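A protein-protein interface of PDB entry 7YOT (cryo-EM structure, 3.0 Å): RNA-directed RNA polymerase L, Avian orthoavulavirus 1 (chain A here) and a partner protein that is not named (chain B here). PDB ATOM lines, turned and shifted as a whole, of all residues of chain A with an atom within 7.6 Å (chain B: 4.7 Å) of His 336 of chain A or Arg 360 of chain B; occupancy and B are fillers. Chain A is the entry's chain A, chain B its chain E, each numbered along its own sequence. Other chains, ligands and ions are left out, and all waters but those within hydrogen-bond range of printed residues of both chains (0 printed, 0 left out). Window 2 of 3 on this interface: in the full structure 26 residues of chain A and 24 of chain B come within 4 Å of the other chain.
OD1 of Asp 357 of chain B lies within hydrogen-bond range of ND1 of His 336 of chain A. The guanidinium group (NH1) of Arg 360 of chain B sits close to a ring nitrogen (ND1) of His 336 of chain A, 3.4 Å away.
The guanidinium group (NE) of Arg 360 of chain B sits at hydrogen-bond distance from the backbone carbonyl oxygen (O) of Arg 356 of chain B, at 3.5 Å. The guanidinium group of Arg 360 of chain B lies within salt-bridge range of the side-chain carboxylate of Asp 357 of chain B (2.4 Å). NE2 of His 336 of chain A lies within hydrogen-bond range of OD1 of Asn 340 of chain A, at 2.9 Å. OG of Ser 343 of chain A lies within hydrogen-bond range of O of Ala 339 of chain A. O of Asn 340 of chain A is in hydrogen-bond range of OG of Ser 343 of chain A, at 3.4 Å.
Among the printed residues, merely in contact across the chains: Leu 299 of chain A with Ala 361 of chain B (3.8 Å), Leu 299 of chain A with Leu 362 of chain B (3.7 Å), Phe 311 of chain A with Thr 358 of chain B (3.6 Å), Phe 311 of chain A with Ala 361 of chain B (3.6 Å), Leu 315 of chain A with Asp 357 of chain B (3.7 Å), Ala 339 of chain A with Asp 357 of chain B (3.6 Å), Ser 343 of chain A with Ala 361 of chain B (3.9 Å) and Ser 343 of chain A with Leu 364 of chain B (3.97 Å).
Printed residues of chain B within 4 Å of Leu 299 of chain A: Ala 361 (3.8 Å) and Leu 362 (3.7 Å). His 336 of chain A touches just these residues of chain B: Asp 357 and Arg 360. Printed residues of chain A within 4 Å of Asp 357 of chain B: Leu 315, His 336 and Ala 339. Printed residues of chain A within 4 Å of Thr 358 of chain B: Phe 311. Of chain A, only His 336 (3.2 Å) comes within 4 Å of Arg 360 of chain B. The nearest printed residue of chain A that does not touch Leu 364 of chain B is Gly 344 of chain A (4.2 Å).
Of the 21 printed residues of chain A, 6 touch a printed residue of chain B. Hydrophobic or aromatic side chains of chain A within 4 Å of the printed part of chain B: Leu 299, Phe 311, Leu 315, His 336 and Ala 339. Along chain A the printed residues that touch a printed residue of chain B span positions 299 to 343. Among the printed residues, 10 pairs touch across the chains. Among the printed residues, no Asp or Glu carboxylate lies within 4 Å of a Lys or Arg side-chain nitrogen of the other chain.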
ATOM      1  N   LEU A 270      -1.526   4.055  -8.071  1.00  0.00           N
ATOM      2  CA  LEU A 270      -0.639   3.660  -6.984  1.00  0.00           C
ATOM      3  C   LEU A 270      -0.556   4.724  -5.903  1.00  0.00           C
ATOM      4  O   LEU A 270      -0.739   4.423  -4.719  1.00  0.00           O
ATOM      5  CB  LEU A 270       0.750   3.366  -7.542  1.00  0.00           C
ATOM      6  CG  LEU A 270       1.853   2.981  -6.564  1.00  0.00           C
ATOM      7  CD1 LEU A 270       1.502   1.718  -5.814  1.00  0.00           C
ATOM      8  CD2 LEU A 270       3.126   2.789  -7.333  1.00  0.00           C
ATOM      9  N   LEU A 299      19.786   9.530 -17.221  1.00  0.00           N
ATOM     10  CA  LEU A 299      20.178   8.179 -17.601  1.00  0.00           C
ATOM     11  C   LEU A 299      20.862   8.168 -18.960  1.00  0.00           C
ATOM     12  O   LEU A 299      21.664   7.276 -19.245  1.00  0.00           O
ATOM     13  CB  LEU A 299      18.955   7.262 -17.624  1.00  0.00           C
ATOM     14  CG  LEU A 299      18.219   6.997 -16.312  1.00  0.00           C
ATOM     15  CD1 LEU A 299      16.958   6.216 -16.548  1.00  0.00           C
ATOM     16  CD2 LEU A 299      19.098   6.258 -15.344  1.00  0.00           C
ATOM     17  N   PHE A 311      18.809   9.792 -10.167  1.00  0.00           N
ATOM     18  CA  PHE A 311      17.785   8.751 -10.165  1.00  0.00           C
ATOM     19  C   PHE A 311      17.908   7.863  -8.934  1.00  0.00           C
ATOM     20  O   PHE A 311      16.918   7.609  -8.236  1.00  0.00           O
ATOM     21  CB  PHE A 311      17.906   7.924 -11.443  1.00  0.00           C
ATOM     22  CG  PHE A 311      16.801   6.935 -11.643  1.00  0.00           C
ATOM     23  CD1 PHE A 311      15.559   7.348 -12.087  1.00  0.00           C
ATOM     24  CD2 PHE A 311      17.007   5.592 -11.415  1.00  0.00           C
ATOM     25  CE1 PHE A 311      14.543   6.440 -12.285  1.00  0.00           C
ATOM     26  CE2 PHE A 311      15.996   4.682 -11.608  1.00  0.00           C
ATOM     27  CZ  PHE A 311      14.763   5.108 -12.044  1.00  0.00           C
ATOM     28  N   LEU A 315      15.409   7.629  -5.684  1.00  0.00           N
ATOM     29  CA  LEU A 315      14.862   6.328  -5.333  1.00  0.00           C
ATOM     30  C   LEU A 315      15.171   5.997  -3.873  1.00  0.00           C
ATOM     31  O   LEU A 315      14.319   5.459  -3.151  1.00  0.00           O
ATOM     32  CB  LEU A 315      15.419   5.291  -6.300  1.00  0.00           C
ATOM     33  CG  LEU A 315      14.650   4.006  -6.525  1.00  0.00           C
ATOM     34  CD1 LEU A 315      13.285   4.359  -7.048  1.00  0.00           C
ATOM     35  CD2 LEU A 315      15.386   3.210  -7.555  1.00  0.00           C
ATOM     36  N   LEU A 318      12.830   8.193  -1.805  1.00  0.00           N
ATOM     37  CA  LEU A 318      11.478   7.656  -1.808  1.00  0.00           C
ATOM     38  C   LEU A 318      11.365   6.472  -0.858  1.00  0.00           C
ATOM     39  O   LEU A 318      10.387   6.370  -0.107  1.00  0.00           O
ATOM     40  CB  LEU A 318      11.093   7.297  -3.243  1.00  0.00           C
ATOM     41  CG  LEU A 318       9.683   6.942  -3.711  1.00  0.00           C
ATOM     42  CD1 LEU A 318       9.424   5.471  -3.649  1.00  0.00           C
ATOM     43  CD2 LEU A 318       8.674   7.684  -2.865  1.00  0.00           C
ATOM     44  N   LEU A 322       9.151   6.417   2.622  1.00  0.00           N
ATOM     45  CA  LEU A 322       8.132   5.390   2.789  1.00  0.00           C
ATOM     46  C   LEU A 322       8.354   4.502   4.007  1.00  0.00           C
ATOM     47  O   LEU A 322       7.374   4.057   4.610  1.00  0.00           O
ATOM     48  CB  LEU A 322       8.039   4.523   1.541  1.00  0.00           C
ATOM     49  CG  LEU A 322       7.352   5.177   0.353  1.00  0.00           C
ATOM     50  CD1 LEU A 322       7.407   4.250  -0.810  1.00  0.00           C
ATOM     51  CD2 LEU A 322       5.926   5.495   0.698  1.00  0.00           C
ATOM     52  N   ILE A 330       6.056  -3.259   1.890  1.00  0.00           N
ATOM     53  CA  ILE A 330       5.272  -2.405   1.011  1.00  0.00           C
ATOM     54  C   ILE A 330       6.111  -1.232   0.520  1.00  0.00           C
ATOM     55  O   ILE A 330       5.960  -0.796  -0.625  1.00  0.00           O
ATOM     56  CB  ILE A 330       3.994  -1.957   1.742  1.00  0.00           C
ATOM     57  CG1 ILE A 330       3.199  -3.184   2.167  1.00  0.00           C
ATOM     58  CG2 ILE A 330       3.104  -1.121   0.842  1.00  0.00           C
ATOM     59  CD1 ILE A 330       2.071  -2.881   3.101  1.00  0.00           C
ATOM     60  N   ALA A 331       7.045  -0.748   1.344  1.00  0.00           N
ATOM     61  CA  ALA A 331       7.969   0.287   0.890  1.00  0.00           C
ATOM     62  C   ALA A 331       8.875  -0.231  -0.219  1.00  0.00           C
ATOM     63  O   ALA A 331       9.123   0.476  -1.205  1.00  0.00           O
ATOM     64  CB  ALA A 331       8.797   0.804   2.061  1.00  0.00           C
ATOM     65  N   ASP A 332       9.331  -1.484  -0.100  1.00  0.00           N
ATOM     66  CA  ASP A 332      10.137  -2.093  -1.154  1.00  0.00           C
ATOM     67  C   ASP A 332       9.345  -2.262  -2.443  1.00  0.00           C
ATOM     68  O   ASP A 332       9.853  -1.967  -3.533  1.00  0.00           O
ATOM     69  CB  ASP A 332      10.660  -3.452  -0.703  1.00  0.00           C
ATOM     70  CG  ASP A 332      11.618  -3.349   0.446  1.00  0.00           C
ATOM     71  OD1 ASP A 332      12.215  -2.276   0.611  1.00  0.00           O
ATOM     72  OD2 ASP A 332      11.781  -4.346   1.179  1.00  0.00           O
ATOM     73  N   SER A 333       8.097  -2.720  -2.339  1.00  0.00           N
ATOM     74  CA  SER A 333       7.307  -2.979  -3.540  1.00  0.00           C
ATOM     75  C   SER A 333       6.892  -1.686  -4.233  1.00  0.00           C
ATOM     76  O   SER A 333       6.908  -1.607  -5.468  1.00  0.00           O
ATOM     77  CB  SER A 333       6.086  -3.823  -3.191  1.00  0.00           C
ATOM     78  OG  SER A 333       5.197  -3.105  -2.361  1.00  0.00           O
ATOM     79  N   VAL A 334       6.553  -0.649  -3.461  1.00  0.00           N
ATOM     80  CA  VAL A 334       6.208   0.637  -4.058  1.00  0.00           C
ATOM     81  C   VAL A 334       7.438   1.293  -4.679  1.00  0.00           C
ATOM     82  O   VAL A 334       7.352   1.854  -5.774  1.00  0.00           O
ATOM     83  CB  VAL A 334       5.518   1.546  -3.022  1.00  0.00           C
ATOM     84  CG1 VAL A 334       5.316   2.939  -3.563  1.00  0.00           C
ATOM     85  CG2 VAL A 334       4.162   0.992  -2.676  1.00  0.00           C
ATOM     86  N   THR A 335       8.607   1.185  -4.029  1.00  0.00           N
ATOM     87  CA  THR A 335       9.838   1.732  -4.604  1.00  0.00           C
ATOM     88  C   THR A 335      10.210   1.021  -5.903  1.00  0.00           C
ATOM     89  O   THR A 335      10.620   1.664  -6.876  1.00  0.00           O
ATOM     90  CB  THR A 335      10.972   1.624  -3.585  1.00  0.00           C
ATOM     91  OG1 THR A 335      10.575   2.258  -2.366  1.00  0.00           O
ATOM     92  CG2 THR A 335      12.206   2.317  -4.084  1.00  0.00           C
ATOM     93  N   HIS A 336      10.003  -0.299  -5.955  1.00  0.00           N
ATOM     94  CA  HIS A 336      10.205  -1.052  -7.188  1.00  0.00           C
ATOM     95  C   HIS A 336       9.232  -0.620  -8.279  1.00  0.00           C
ATOM     96  O   HIS A 336       9.607  -0.529  -9.457  1.00  0.00           O
ATOM     97  CB  HIS A 336      10.055  -2.541  -6.899  1.00  0.00           C
ATOM     98  CG  HIS A 336      10.228  -3.410  -8.100  1.00  0.00           C
ATOM     99  ND1 HIS A 336      11.462  -3.695  -8.640  1.00  0.00           N
ATOM    100  CD2 HIS A 336       9.322  -4.048  -8.874  1.00  0.00           C
ATOM    101  CE1 HIS A 336      11.310  -4.481  -9.688  1.00  0.00           C
ATOM    102  NE2 HIS A 336      10.020  -4.705  -9.857  1.00  0.00           N
ATOM    103  N   ALA A 337       7.982  -0.330  -7.907  1.00  0.00           N
ATOM    104  CA  ALA A 337       6.993   0.112  -8.886  1.00  0.00           C
ATOM    105  C   ALA A 337       7.334   1.483  -9.458  1.00  0.00           C
ATOM    106  O   ALA A 337       7.242   1.687 -10.677  1.00  0.00           O
ATOM    107  CB  ALA A 337       5.605   0.128  -8.256  1.00  0.00           C
ATOM    108  N   ILE A 338       7.744   2.427  -8.601  1.00  0.00           N
ATOM    109  CA  ILE A 338       8.166   3.750  -9.069  1.00  0.00           C
ATOM    110  C   ILE A 338       9.406   3.629  -9.945  1.00  0.00           C
ATOM    111  O   ILE A 338       9.558   4.360 -10.930  1.00  0.00           O
ATOM    112  CB  ILE A 338       8.436   4.709  -7.888  1.00  0.00           C
ATOM    113  CG1 ILE A 338       7.262   4.793  -6.922  1.00  0.00           C
ATOM    114  CG2 ILE A 338       8.721   6.111  -8.373  1.00  0.00           C
ATOM    115  CD1 ILE A 338       6.015   5.227  -7.501  1.00  0.00           C
ATOM    116  N   ALA A 339      10.298   2.694  -9.619  1.00  0.00           N
ATOM    117  CA  ALA A 339      11.505   2.516 -10.411  1.00  0.00           C
ATOM    118  C   ALA A 339      11.200   1.941 -11.785  1.00  0.00           C
ATOM    119  O   ALA A 339      11.874   2.279 -12.761  1.00  0.00           O
ATOM    120  CB  ALA A 339      12.478   1.618  -9.667  1.00  0.00           C
ATOM    121  N   ASN A 340      10.200   1.070 -11.887  1.00  0.00           N
ATOM    122  CA  ASN A 340       9.843   0.540 -13.199  1.00  0.00           C
ATOM    123  C   ASN A 340       8.952   1.463 -14.012  1.00  0.00           C
ATOM    124  O   ASN A 340       8.853   1.270 -15.225  1.00  0.00           O
ATOM    125  CB  ASN A 340       9.153  -0.813 -13.077  1.00  0.00           C
ATOM    126  CG  ASN A 340      10.104  -1.911 -12.706  1.00  0.00           C
ATOM    127  OD1 ASN A 340      10.040  -2.451 -11.611  1.00  0.00           O
ATOM    128  ND2 ASN A 340      10.991  -2.265 -13.628  1.00  0.00           N
ATOM    129  N   ILE A 341       8.278   2.433 -13.393  1.00  0.00           N
ATOM    130  CA  ILE A 341       7.480   3.367 -14.187  1.00  0.00           C
ATOM    131  C   ILE A 341       8.383   4.336 -14.945  1.00  0.00           C
ATOM    132  O   ILE A 341       8.265   4.486 -16.165  1.00  0.00           O
ATOM    133  CB  ILE A 341       6.450   4.096 -13.304  1.00  0.00           C
ATOM    134  CG1 ILE A 341       5.322   3.137 -12.933  1.00  0.00           C
ATOM    135  CG2 ILE A 341       5.885   5.303 -14.009  1.00  0.00           C
ATOM    136  CD1 ILE A 341       4.423   3.628 -11.850  1.00  0.00           C
ATOM    137  N   PHE A 342       9.328   4.963 -14.255  1.00  0.00           N
ATOM    138  CA  PHE A 342      10.191   5.962 -14.872  1.00  0.00           C
ATOM    139  C   PHE A 342      11.380   5.377 -15.628  1.00  0.00           C
ATOM    140  O   PHE A 342      12.295   6.131 -15.961  1.00  0.00           O
ATOM    141  CB  PHE A 342      10.701   6.938 -13.816  1.00  0.00           C
ATOM    142  CG  PHE A 342       9.656   7.878 -13.305  1.00  0.00           C
ATOM    143  CD1 PHE A 342       9.339   9.025 -14.000  1.00  0.00           C
ATOM    144  CD2 PHE A 342       8.985   7.611 -12.132  1.00  0.00           C
ATOM    145  CE1 PHE A 342       8.380   9.891 -13.521  1.00  0.00           C
ATOM    146  CE2 PHE A 342       8.025   8.470 -11.658  1.00  0.00           C
ATOM    147  CZ  PHE A 342       7.724   9.610 -12.354  1.00  0.00           C
ATOM    148  N   SER A 343      11.408   4.084 -15.926  1.00  0.00           N
ATOM    149  CA  SER A 343      12.531   3.479 -16.627  1.00  0.00           C
ATOM    150  C   SER A 343      12.091   2.972 -17.990  1.00  0.00           C
ATOM    151  O   SER A 343      11.010   2.397 -18.130  1.00  0.00           O
ATOM    152  CB  SER A 343      13.133   2.330 -15.834  1.00  0.00           C
ATOM    153  OG  SER A 343      12.229   1.249 -15.754  1.00  0.00           O
ATOM    154  N   GLY A 344      12.944   3.170 -18.985  1.00  0.00           N
ATOM    155  CA  GLY A 344      12.634   2.819 -20.349  1.00  0.00           C
ATOM    156  C   GLY A 344      12.184   3.972 -21.210  1.00  0.00           C
ATOM    157  O   GLY A 344      11.688   3.736 -22.316  1.00  0.00           O
ATOM    158  N   ARG B 356      19.939  -2.303  -7.901  1.00  0.00           N
ATOM    159  CA  ARG B 356      19.486  -3.130  -9.011  1.00  0.00           C
ATOM    160  C   ARG B 356      18.456  -2.417  -9.884  1.00  0.00           C
ATOM    161  O   ARG B 356      18.455  -2.597 -11.109  1.00  0.00           O
ATOM    162  CB  ARG B 356      18.923  -4.450  -8.475  1.00  0.00           C
ATOM    163  CG  ARG B 356      18.541  -5.462  -9.541  1.00  0.00           C
ATOM    164  CD  ARG B 356      18.070  -6.772  -8.930  1.00  0.00           C
ATOM    165  NE  ARG B 356      19.152  -7.492  -8.266  1.00  0.00           N
ATOM    166  CZ  ARG B 356      18.984  -8.587  -7.535  1.00  0.00           C
ATOM    167  NH1 ARG B 356      20.027  -9.174  -6.971  1.00  0.00           N
ATOM    168  NH2 ARG B 356      17.774  -9.100  -7.372  1.00  0.00           N
ATOM    169  N   ASP B 357      17.607  -1.576  -9.284  1.00  0.00           N
ATOM    170  CA  ASP B 357      16.629  -0.816 -10.057  1.00  0.00           C
ATOM    171  C   ASP B 357      17.296   0.221 -10.947  1.00  0.00           C
ATOM    172  O   ASP B 357      16.866   0.436 -12.087  1.00  0.00           O
ATOM    173  CB  ASP B 357      15.638  -0.135  -9.124  1.00  0.00           C
ATOM    174  CG  ASP B 357      14.629  -1.093  -8.544  1.00  0.00           C
ATOM    175  OD1 ASP B 357      14.331  -2.109  -9.205  1.00  0.00           O
ATOM    176  OD2 ASP B 357      14.117  -0.821  -7.437  1.00  0.00           O
ATOM    177  N   THR B 358      18.350   0.867 -10.453  1.00  0.00           N
ATOM    178  CA  THR B 358      19.033   1.858 -11.270  1.00  0.00           C
ATOM    179  C   THR B 358      19.788   1.212 -12.416  1.00  0.00           C
ATOM    180  O   THR B 358      19.815   1.757 -13.514  1.00  0.00           O
ATOM    181  CB  THR B 358      19.980   2.702 -10.430  1.00  0.00           C
ATOM    182  OG1 THR B 358      20.902   1.851  -9.743  1.00  0.00           O
ATOM    183  CG2 THR B 358      19.202   3.506  -9.447  1.00  0.00           C
ATOM    184  N   VAL B 359      20.373   0.036 -12.204  1.00  0.00           N
ATOM    185  CA  VAL B 359      21.089  -0.573 -13.314  1.00  0.00           C
ATOM    186  C   VAL B 359      20.104  -1.191 -14.307  1.00  0.00           C
ATOM    187  O   VAL B 359      20.391  -1.253 -15.509  1.00  0.00           O
ATOM    188  CB  VAL B 359      22.152  -1.563 -12.791  1.00  0.00           C
ATOM    189  CG1 VAL B 359      21.529  -2.781 -12.180  1.00  0.00           C
ATOM    190  CG2 VAL B 359      23.151  -1.928 -13.881  1.00  0.00           C
ATOM    191  N   ARG B 360      18.893  -1.558 -13.860  1.00  0.00           N
ATOM    192  CA  ARG B 360      17.833  -1.861 -14.822  1.00  0.00           C
ATOM    193  C   ARG B 360      17.412  -0.629 -15.607  1.00  0.00           C
ATOM    194  O   ARG B 360      17.124  -0.723 -16.802  1.00  0.00           O
ATOM    195  CB  ARG B 360      16.619  -2.482 -14.133  1.00  0.00           C
ATOM    196  CG  ARG B 360      16.767  -3.962 -13.922  1.00  0.00           C
ATOM    197  CD  ARG B 360      15.575  -4.623 -13.264  1.00  0.00           C
ATOM    198  NE  ARG B 360      15.500  -4.317 -11.843  1.00  0.00           N
ATOM    199  CZ  ARG B 360      14.570  -4.800 -11.033  1.00  0.00           C
ATOM    200  NH1 ARG B 360      14.571  -4.475  -9.750  1.00  0.00           N
ATOM    201  NH2 ARG B 360      13.653  -5.628 -11.506  1.00  0.00           N
ATOM    202  N   ALA B 361      17.373   0.534 -14.960  1.00  0.00           N
ATOM    203  CA  ALA B 361      17.035   1.760 -15.676  1.00  0.00           C
ATOM    204  C   ALA B 361      18.125   2.140 -16.669  1.00  0.00           C
ATOM    205  O   ALA B 361      17.831   2.671 -17.743  1.00  0.00           O
ATOM    206  CB  ALA B 361      16.789   2.894 -14.687  1.00  0.00           C
ATOM    207  N   LEU B 362      19.388   1.869 -16.333  1.00  0.00           N
ATOM    208  CA  LEU B 362      20.479   2.153 -17.260  1.00  0.00           C
ATOM    209  C   LEU B 362      20.474   1.193 -18.445  1.00  0.00           C
ATOM    210  O   LEU B 362      20.775   1.601 -19.570  1.00  0.00           O
ATOM    211  CB  LEU B 362      21.836   2.108 -16.551  1.00  0.00           C
ATOM    212  CG  LEU B 362      22.484   3.361 -15.933  1.00  0.00           C
ATOM    213  CD1 LEU B 362      22.491   4.493 -16.919  1.00  0.00           C
ATOM    214  CD2 LEU B 362      21.940   3.851 -14.626  1.00  0.00           C
ATOM    215  N   ILE B 363      20.140  -0.081 -18.224  1.00  0.00           N
ATOM    216  CA  ILE B 363      20.095  -1.023 -19.342  1.00  0.00           C
ATOM    217  C   ILE B 363      18.883  -0.752 -20.232  1.00  0.00           C
ATOM    218  O   ILE B 363      18.984  -0.776 -21.464  1.00  0.00           O
ATOM    219  CB  ILE B 363      20.122  -2.473 -18.822  1.00  0.00           C
ATOM    220  CG1 ILE B 363      21.463  -2.774 -18.160  1.00  0.00           C
ATOM    221  CG2 ILE B 363      19.913  -3.468 -19.940  1.00  0.00           C
ATOM    222  CD1 ILE B 363      21.469  -4.065 -17.380  1.00  0.00           C
ATOM    223  N   LEU B 364      17.729  -0.451 -19.629  1.00  0.00           N
ATOM    224  CA  LEU B 364      16.506  -0.261 -20.404  1.00  0.00           C
ATOM    225  C   LEU B 364      16.490   1.048 -21.186  1.00  0.00           C
ATOM    226  O   LEU B 364      15.973   1.083 -22.306  1.00  0.00           O
ATOM    227  CB  LEU B 364      15.285  -0.331 -19.488  1.00  0.00           C
ATOM    228  CG  LEU B 364      14.546  -1.660 -19.320  1.00  0.00           C
ATOM    229  CD1 LEU B 364      15.379  -2.722 -18.673  1.00  0.00           C
ATOM    230  CD2 LEU B 364      13.305  -1.412 -18.490  1.00  0.00           C
ATOM    231  N   LEU B 377      20.249  -7.985 -19.099  1.00  0.00           N
ATOM    232  CA  LEU B 377      19.120  -8.214 -18.205  1.00  0.00           C
ATOM    233  C   LEU B 377      19.051  -9.662 -17.748  1.00  0.00           C
ATOM    234  O   LEU B 377      18.462  -9.951 -16.701  1.00  0.00           O
ATOM    235  CB  LEU B 377      17.814  -7.823 -18.884  1.00  0.00           C
ATOM    236  CG  LEU B 377      17.557  -6.333 -19.053  1.00  0.00           C
ATOM    237  CD1 LEU B 377      16.326  -6.121 -19.905  1.00  0.00           C
ATOM    238  CD2 LEU B 377      17.389  -5.698 -17.686  1.00  0.00           C
ATOM    239  N   LEU B 380      21.355 -10.390 -14.470  1.00  0.00           N
ATOM    240  CA  LEU B 380      21.181  -9.332 -13.484  1.00  0.00           C
ATOM    241  C   LEU B 380      20.215  -9.800 -12.407  1.00  0.00           C
ATOM    242  O   LEU B 380      20.336  -9.418 -11.239  1.00  0.00           O
ATOM    243  CB  LEU B 380      20.698  -8.045 -14.155  1.00  0.00           C
ATOM    244  CG  LEU B 380      20.404  -6.830 -13.274  1.00  0.00           C
ATOM    245  CD1 LEU B 380      21.590  -6.488 -12.417  1.00  0.00           C
ATOM    246  CD2 LEU B 380      20.058  -5.651 -14.143  1.00  0.00           C
